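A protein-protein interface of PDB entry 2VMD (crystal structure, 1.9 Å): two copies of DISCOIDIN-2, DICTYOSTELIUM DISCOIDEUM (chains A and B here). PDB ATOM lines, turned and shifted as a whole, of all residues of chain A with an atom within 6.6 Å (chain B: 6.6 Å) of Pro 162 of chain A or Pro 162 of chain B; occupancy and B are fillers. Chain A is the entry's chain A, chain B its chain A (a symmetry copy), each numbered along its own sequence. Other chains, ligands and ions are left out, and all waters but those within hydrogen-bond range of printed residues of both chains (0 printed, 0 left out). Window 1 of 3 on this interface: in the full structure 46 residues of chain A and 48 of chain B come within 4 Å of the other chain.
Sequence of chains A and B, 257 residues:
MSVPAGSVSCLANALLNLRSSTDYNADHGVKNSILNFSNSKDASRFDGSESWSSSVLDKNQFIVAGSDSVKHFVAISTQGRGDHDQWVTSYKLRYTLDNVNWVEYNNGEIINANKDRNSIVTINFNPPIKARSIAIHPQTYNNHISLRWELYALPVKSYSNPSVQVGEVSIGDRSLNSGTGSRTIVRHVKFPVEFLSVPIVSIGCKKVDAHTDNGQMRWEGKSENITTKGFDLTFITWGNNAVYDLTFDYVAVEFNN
Tyr 159 of chain A touches Ser 163 of chain B.
OH of Tyr 159 of chain A touches OE1 of Glu 254 of chain B, 3.7 Å away.
CA of Ser 160 of chain A touches OG of Ser 163 of chain B, at 3.8 Å.
O of Pro 162 of chain B touches CD of Pro 162 of chain A, at 3.3 Å.
Pro 162 of chain A touches Val 164 of chain B.
Val 164 of chain B touches Phe 255 of chain A (O to CE1, 3.0 Å).
ND2 of Asn 161 of chain A lies close to ND2 of Asn 161 of chain B (3.3 Å).
N of Val 164 of chain B sits at hydrogen-bond distance from O of Tyr 159 of chain A, 3.4 Å away.
Of the 11 printed residues of chain B, 5 touch a printed residue of chain A.
Among the printed residues, no Asp or Glu carboxylate lies within 4 Å of a Lys or Arg side-chain nitrogen of the other chain.
Tyr 159 of chain A touches Ser 163 of chain B, but with the chains exchanged Ser 163 of chain A does not touch Tyr 159 of chain B (12.2 Å).
Asn 161 of chain A touches its own counterpart, Asn 161 of chain B.
Pro 162 of chain A touches its own counterpart, Pro 162 of chain B.
Phe 255 of chain A touches Val 164 of chain B, but with the chains exchanged Val 164 of chain A does not touch Phe 255 of chain B (11.1 Å).
Of the 8 pairs that touch across the chains among the printed residues, 2 have their exchanged pair printed and touching as well.
The backbone carbonyl oxygen of Ser 163 of chain B sits at hydrogen-bond distance from the backbone NH of Glu 254 of chain B.
Of chain B, only Pro 162 (3.3 Å) and Val 164 (3.9 Å) come within 4 Å of Pro 162 of chain A.
Of the printed residues of chain A, Ser 163 of chain B touches Tyr 159 and Ser 160.
Printed residues of chain A within 4 Å of Asn 161 of chain B: Asn 161.
Of the printed residues of chain B, Phe 255 of chain A touches Val 164.
Printed residues of chain A within 4 Å of Val 164 of chain B: Tyr 159, Pro 162 and Phe 255.
Of the printed residues of chain B, Tyr 159 of chain A touches Ser 163, Val 164 and Glu 254.
Glu 254 of chain A touches none of the printed residues of chain B.
Val 164 of chain A touches none of the printed residues of chain B.
The nearest residue of chain B that does not touch Pro 162 of chain A is Ser 163 of chain B (4.5 Å).
The nearest printed residue of chain A that does not touch Asn 161 of chain B is Pro 162 of chain A (5.9 Å).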
ATOM      1  N   TYR A 159      23.168  28.841  10.949  1.00  0.00           N
ATOM      2  CA  TYR A 159      23.798  27.678  11.585  1.00  0.00           C
ATOM      3  C   TYR A 159      23.335  27.359  13.020  1.00  0.00           C
ATOM      4  O   TYR A 159      23.899  26.470  13.651  1.00  0.00           O
ATOM      5  CB  TYR A 159      25.328  27.835  11.564  1.00  0.00           C
ATOM      6  CG  TYR A 159      25.849  29.086  12.254  1.00  0.00           C
ATOM      7  CD1 TYR A 159      25.631  29.296  13.619  1.00  0.00           C
ATOM      8  CD2 TYR A 159      26.563  30.048  11.551  1.00  0.00           C
ATOM      9  CE1 TYR A 159      26.108  30.441  14.267  1.00  0.00           C
ATOM     10  CE2 TYR A 159      27.050  31.196  12.183  1.00  0.00           C
ATOM     11  CZ  TYR A 159      26.814  31.387  13.544  1.00  0.00           C
ATOM     12  OH  TYR A 159      27.284  32.517  14.206  1.00  0.00           O
ATOM     13  N   SER A 160      22.342  28.080  13.549  1.00  0.00           N
ATOM     14  CA  SER A 160      21.972  27.895  14.973  1.00  0.00           C
ATOM     15  C   SER A 160      20.947  26.795  15.191  1.00  0.00           C
ATOM     16  O   SER A 160      20.133  26.494  14.318  1.00  0.00           O
ATOM     17  CB  SER A 160      21.469  29.188  15.619  1.00  0.00           C
ATOM     18  OG  SER A 160      21.748  30.297  14.784  1.00  0.00           O
ATOM     19  N   ASN A 161      20.989  26.195  16.374  1.00  0.00           N
ATOM     20  CA  ASN A 161      20.011  25.176  16.744  1.00  0.00           C
ATOM     21  C   ASN A 161      19.892  24.041  15.711  1.00  0.00           C
ATOM     22  O   ASN A 161      18.783  23.678  15.288  1.00  0.00           O
ATOM     23  CB  ASN A 161      18.645  25.835  17.035  1.00  0.00           C
ATOM     24  CG  ASN A 161      18.736  26.931  18.095  1.00  0.00           C
ATOM     25  OD1 ASN A 161      18.811  28.131  17.776  1.00  0.00           O
ATOM     26  ND2 ASN A 161      18.770  26.519  19.371  1.00  0.00           N
ATOM     27  N   PRO A 162      21.041  23.449  15.316  1.00  0.00           N
ATOM     28  CA  PRO A 162      20.977  22.352  14.363  1.00  0.00           C
ATOM     29  C   PRO A 162      20.493  21.075  15.030  1.00  0.00           C
ATOM     30  O   PRO A 162      20.625  20.914  16.238  1.00  0.00           O
ATOM     31  CB  PRO A 162      22.430  22.188  13.939  1.00  0.00           C
ATOM     32  CG  PRO A 162      23.189  22.530  15.199  1.00  0.00           C
ATOM     33  CD  PRO A 162      22.424  23.718  15.748  1.00  0.00           C
ATOM     34  N   SER A 163      19.909  20.193  14.237  1.00  0.00           N
ATOM     35  CA  SER A 163      19.550  18.870  14.682  1.00  0.00           C
ATOM     36  C   SER A 163      20.692  17.913  14.289  1.00  0.00           C
ATOM     37  O   SER A 163      21.359  18.122  13.285  1.00  0.00           O
ATOM     38  CB  SER A 163      18.240  18.434  14.021  1.00  0.00           C
ATOM     39  OG  SER A 163      17.137  19.295  14.369  1.00  0.00           O
ATOM     40  N   VAL A 164      20.897  16.868  15.085  1.00  0.00           N
ATOM     41  CA  VAL A 164      22.044  15.971  14.916  1.00  0.00           C
ATOM     42  C   VAL A 164      21.656  14.506  15.090  1.00  0.00           C
ATOM     43  O   VAL A 164      20.901  14.158  15.990  1.00  0.00           O
ATOM     44  CB  VAL A 164      23.127  16.306  15.948  1.00  0.00           C
ATOM     45  CG1 VAL A 164      24.226  15.269  15.921  1.00  0.00           C
ATOM     46  CG2 VAL A 164      23.682  17.688  15.703  1.00  0.00           C
ATOM     47  N   VAL A 253      24.190  16.442  10.368  1.00  0.00           N
ATOM     48  CA  VAL A 253      23.675  17.700  10.915  1.00  0.00           C
ATOM     49  C   VAL A 253      22.611  18.332  10.004  1.00  0.00           C
ATOM     50  O   VAL A 253      22.874  18.594   8.849  1.00  0.00           O
ATOM     51  CB  VAL A 253      24.827  18.709  11.165  1.00  0.00           C
ATOM     52  CG1 VAL A 253      24.303  19.987  11.812  1.00  0.00           C
ATOM     53  CG2 VAL A 253      25.945  18.070  12.015  1.00  0.00           C
ATOM     54  N   GLU A 254      21.418  18.587  10.557  1.00  0.00           N
ATOM     55  CA  GLU A 254      20.363  19.318   9.857  1.00  0.00           C
ATOM     56  C   GLU A 254      20.248  20.767  10.346  1.00  0.00           C
ATOM     57  O   GLU A 254      20.099  21.016  11.527  1.00  0.00           O
ATOM     58  CB  GLU A 254      19.027  18.585   9.997  1.00  0.00           C
ATOM     59  CG  GLU A 254      17.918  19.210   9.168  1.00  0.00           C
ATOM     60  CD  GLU A 254      16.545  18.771   9.612  1.00  0.00           C
ATOM     61  OE1 GLU A 254      16.319  18.594  10.827  1.00  0.00           O
ATOM     62  OE2 GLU A 254      15.686  18.609   8.728  1.00  0.00           O
ATOM     63  N   PHE A 255      20.352  21.706   9.415  1.00  0.00           N
ATOM     64  CA  PHE A 255      20.256  23.121   9.688  1.00  0.00           C
ATOM     65  C   PHE A 255      18.882  23.676   9.326  1.00  0.00           C
ATOM     66  O   PHE A 255      18.175  23.122   8.469  1.00  0.00           O
ATOM     67  CB  PHE A 255      21.294  23.870   8.865  1.00  0.00           C
ATOM     68  CG  PHE A 255      22.695  23.474   9.162  1.00  0.00           C
ATOM     69  CD1 PHE A 255      23.377  24.056  10.223  1.00  0.00           C
ATOM     70  CD2 PHE A 255      23.336  22.506   8.385  1.00  0.00           C
ATOM     71  CE1 PHE A 255      24.684  23.686  10.518  1.00  0.00           C
ATOM     72  CE2 PHE A 255      24.658  22.115   8.679  1.00  0.00           C
ATOM     73  CZ  PHE A 255      25.329  22.712   9.738  1.00  0.00           C
ATOM     74  N   ASN A 256      18.513  24.773   9.981  1.00  0.00           N
ATOM     75  CA  ASN A 256      17.366  25.587   9.550  1.00  0.00           C
ATOM     76  C   ASN A 256      16.009  24.961   9.801  1.00  0.00           C
ATOM     77  O   ASN A 256      15.046  25.298   9.106  1.00  0.00           O
ATOM     78  CB  ASN A 256      17.468  25.873   8.038  1.00  0.00           C
ATOM     79  CG  ASN A 256      18.230  27.121   7.739  1.00  0.00           C
ATOM     80  OD1 ASN A 256      19.368  27.070   7.222  1.00  0.00           O
ATOM     81  ND2 ASN A 256      17.614  28.275   8.055  1.00  0.00           N
ATOM     82  N   ASN A 257      15.909  24.046  10.755  1.00  0.00           N
ATOM     83  CA  ASN A 257      14.647  23.334  10.933  1.00  0.00           C
ATOM     84  C   ASN A 257      14.301  23.150  12.406  1.00  0.00           C
ATOM     85  O   ASN A 257      14.906  23.813  13.286  1.00  0.00           O
ATOM     86  CB  ASN A 257      14.646  21.992  10.159  1.00  0.00           C
ATOM     87  CG  ASN A 257      14.032  22.102   8.746  1.00  0.00           C
ATOM     88  OD1 ASN A 257      13.243  21.253   8.346  1.00  0.00           O
ATOM     89  ND2 ASN A 257      14.398  23.128   7.992  1.00  0.00           N
ATOM     90  OXT ASN A 257      13.397  22.353  12.737  1.00  0.00           O
ATOM     91  N   TYR B 159      26.850  24.187  27.765  1.00  0.00           N
ATOM     92  CA  TYR B 159      26.975  23.410  26.526  1.00  0.00           C
ATOM     93  C   TYR B 159      25.691  23.269  25.685  1.00  0.00           C
ATOM     94  O   TYR B 159      25.697  22.541  24.696  1.00  0.00           O
ATOM     95  CB  TYR B 159      27.536  22.013  26.840  1.00  0.00           C
ATOM     96  CG  TYR B 159      26.709  21.199  27.823  1.00  0.00           C
ATOM     97  CD1 TYR B 159      25.392  20.838  27.524  1.00  0.00           C
ATOM     98  CD2 TYR B 159      27.242  20.786  29.037  1.00  0.00           C
ATOM     99  CE1 TYR B 159      24.620  20.086  28.418  1.00  0.00           C
ATOM    100  CE2 TYR B 159      26.485  20.031  29.941  1.00  0.00           C
ATOM    101  CZ  TYR B 159      25.172  19.689  29.624  1.00  0.00           C
ATOM    102  OH  TYR B 159      24.391  18.939  30.498  1.00  0.00           O
ATOM    103  N   SER B 160      24.595  23.928  26.070  1.00  0.00           N
ATOM    104  CA  SER B 160      23.310  23.702  25.367  1.00  0.00           C
ATOM    105  C   SER B 160      23.116  24.602  24.160  1.00  0.00           C
ATOM    106  O   SER B 160      23.644  25.712  24.095  1.00  0.00           O
ATOM    107  CB  SER B 160      22.103  23.840  26.298  1.00  0.00           C
ATOM    108  OG  SER B 160      22.522  23.869  27.650  1.00  0.00           O
ATOM    109  N   ASN B 161      22.345  24.115  23.195  1.00  0.00           N
ATOM    110  CA  ASN B 161      22.013  24.906  22.015  1.00  0.00           C
ATOM    111  C   ASN B 161      23.247  25.486  21.302  1.00  0.00           C
ATOM    112  O   ASN B 161      23.300  26.686  20.993  1.00  0.00           O
ATOM    113  CB  ASN B 161      20.995  26.007  22.387  1.00  0.00           C
ATOM    114  CG  ASN B 161      19.739  25.444  23.052  1.00  0.00           C
ATOM    115  OD1 ASN B 161      19.609  25.448  24.289  1.00  0.00           O
ATOM    116  ND2 ASN B 161      18.819  24.918  22.231  1.00  0.00           N
ATOM    117  N   PRO B 162      24.244  24.623  21.005  1.00  0.00           N
ATOM    118  CA  PRO B 162      25.420  25.118  20.305  1.00  0.00           C
ATOM    119  C   PRO B 162      25.121  25.350  18.833  1.00  0.00           C
ATOM    120  O   PRO B 162      24.207  24.751  18.280  1.00  0.00           O
ATOM    121  CB  PRO B 162      26.408  23.969  20.451  1.00  0.00           C
ATOM    122  CG  PRO B 162      25.515  22.750  20.413  1.00  0.00           C
ATOM    123  CD  PRO B 162      24.326  23.173  21.252  1.00  0.00           C
ATOM    124  N   SER B 163      25.880  26.246  18.223  1.00  0.00           N
ATOM    125  CA  SER B 163      25.835  26.457  16.798  1.00  0.00           C
ATOM    126  C   SER B 163      26.959  25.617  16.162  1.00  0.00           C
ATOM    127  O   SER B 163      27.997  25.403  16.773  1.00  0.00           O
ATOM    128  CB  SER B 163      26.036  27.941  16.483  1.00  0.00           C
ATOM    129  OG  SER B 163      25.001  28.767  17.051  1.00  0.00           O
ATOM    130  N   VAL B 164      26.739  25.157  14.933  1.00  0.00           N
ATOM    131  CA  VAL B 164      27.653  24.220  14.275  1.00  0.00           C
ATOM    132  C   VAL B 164      27.878  24.574  12.807  1.00  0.00           C
ATOM    133  O   VAL B 164      26.944  24.917  12.093  1.00  0.00           O
ATOM    134  CB  VAL B 164      27.084  22.798  14.344  1.00  0.00           C
ATOM    135  CG1 VAL B 164      27.909  21.853  13.501  1.00  0.00           C
ATOM    136  CG2 VAL B 164      27.015  22.325  15.775  1.00  0.00           C
ATOM    137  N   VAL B 253      32.180  24.072  16.509  1.00  0.00           N
ATOM    138  CA  VAL B 253      31.065  24.263  17.440  1.00  0.00           C
ATOM    139  C   VAL B 253      31.192  25.572  18.232  1.00  0.00           C
ATOM    140  O   VAL B 253      32.181  25.785  18.904  1.00  0.00           O
ATOM    141  CB  VAL B 253      30.945  23.062  18.415  1.00  0.00           C
ATOM    142  CG1 VAL B 253      29.733  23.219  19.328  1.00  0.00           C
ATOM    143  CG2 VAL B 253      30.892  21.727  17.642  1.00  0.00           C
ATOM    144  N   GLU B 254      30.165  26.427  18.155  1.00  0.00           N
ATOM    145  CA  GLU B 254      30.082  27.639  18.968  1.00  0.00           C
ATOM    146  C   GLU B 254      29.104  27.479  20.138  1.00  0.00           C
ATOM    147  O   GLU B 254      27.956  27.127  19.948  1.00  0.00           O
ATOM    148  CB  GLU B 254      29.701  28.839  18.096  1.00  0.00           C
ATOM    149  CG  GLU B 254      29.744  30.157  18.850  1.00  0.00           C
ATOM    150  CD  GLU B 254      28.987  31.253  18.143  1.00  0.00           C
ATOM    151  OE1 GLU B 254      27.932  30.978  17.535  1.00  0.00           O
ATOM    152  OE2 GLU B 254      29.456  32.402  18.209  1.00  0.00           O
ATOM    153  N   PHE B 255      29.598  27.716  21.347  1.00  0.00           N
ATOM    154  CA  PHE B 255      28.823  27.627  22.562  1.00  0.00           C
ATOM    155  C   PHE B 255      28.391  29.001  23.062  1.00  0.00           C
ATOM    156  O   PHE B 255      29.037  30.019  22.766  1.00  0.00           O
ATOM    157  CB  PHE B 255      29.659  26.975  23.654  1.00  0.00           C
ATOM    158  CG  PHE B 255      30.099  25.593  23.327  1.00  0.00           C
ATOM    159  CD1 PHE B 255      29.260  24.515  23.575  1.00  0.00           C
ATOM    160  CD2 PHE B 255      31.356  25.366  22.761  1.00  0.00           C
ATOM    161  CE1 PHE B 255      29.655  23.219  23.265  1.00  0.00           C
ATOM    162  CE2 PHE B 255      31.765  24.058  22.433  1.00  0.00           C
ATOM    163  CZ  PHE B 255      30.918  22.990  22.693  1.00  0.00           C
ATOM    164  N   ASN B 256      27.298  29.024  23.819  1.00  0.00           N
ATOM    165  CA  ASN B 256      26.923  30.207  24.607  1.00  0.00           C
ATOM    166  C   ASN B 256      26.401  31.376  23.796  1.00  0.00           C
ATOM    167  O   ASN B 256      26.490  32.519  24.248  1.00  0.00           O
ATOM    168  CB  ASN B 256      28.141  30.710  25.407  1.00  0.00           C
ATOM    169  CG  ASN B 256      28.247  30.075  26.754  1.00  0.00           C
ATOM    170  OD1 ASN B 256      29.149  29.247  27.004  1.00  0.00           O
ATOM    171  ND2 ASN B 256      27.325  30.457  27.656  1.00  0.00           N
ATOM    172  N   ASN B 257      25.881  31.124  22.602  1.00  0.00           N
ATOM    173  CA  ASN B 257      25.489  32.240  21.745  1.00  0.00           C
ATOM    174  C   ASN B 257      24.172  31.970  21.027  1.00  0.00           C
ATOM    175  O   ASN B 257      23.427  31.031  21.406  1.00  0.00           O
ATOM    176  CB  ASN B 257      26.624  32.616  20.760  1.00  0.00           C
ATOM    177  CG  ASN B 257      27.542  33.742  21.287  1.00  0.00           C
ATOM    178  OD1 ASN B 257      27.875  34.664  20.551  1.00  0.00           O
ATOM    179  ND2 ASN B 257      27.957  33.664  22.543  1.00  0.00           N
ATOM    180  OXT ASN B 257      23.821  32.700  20.075  1.00  0.00           O
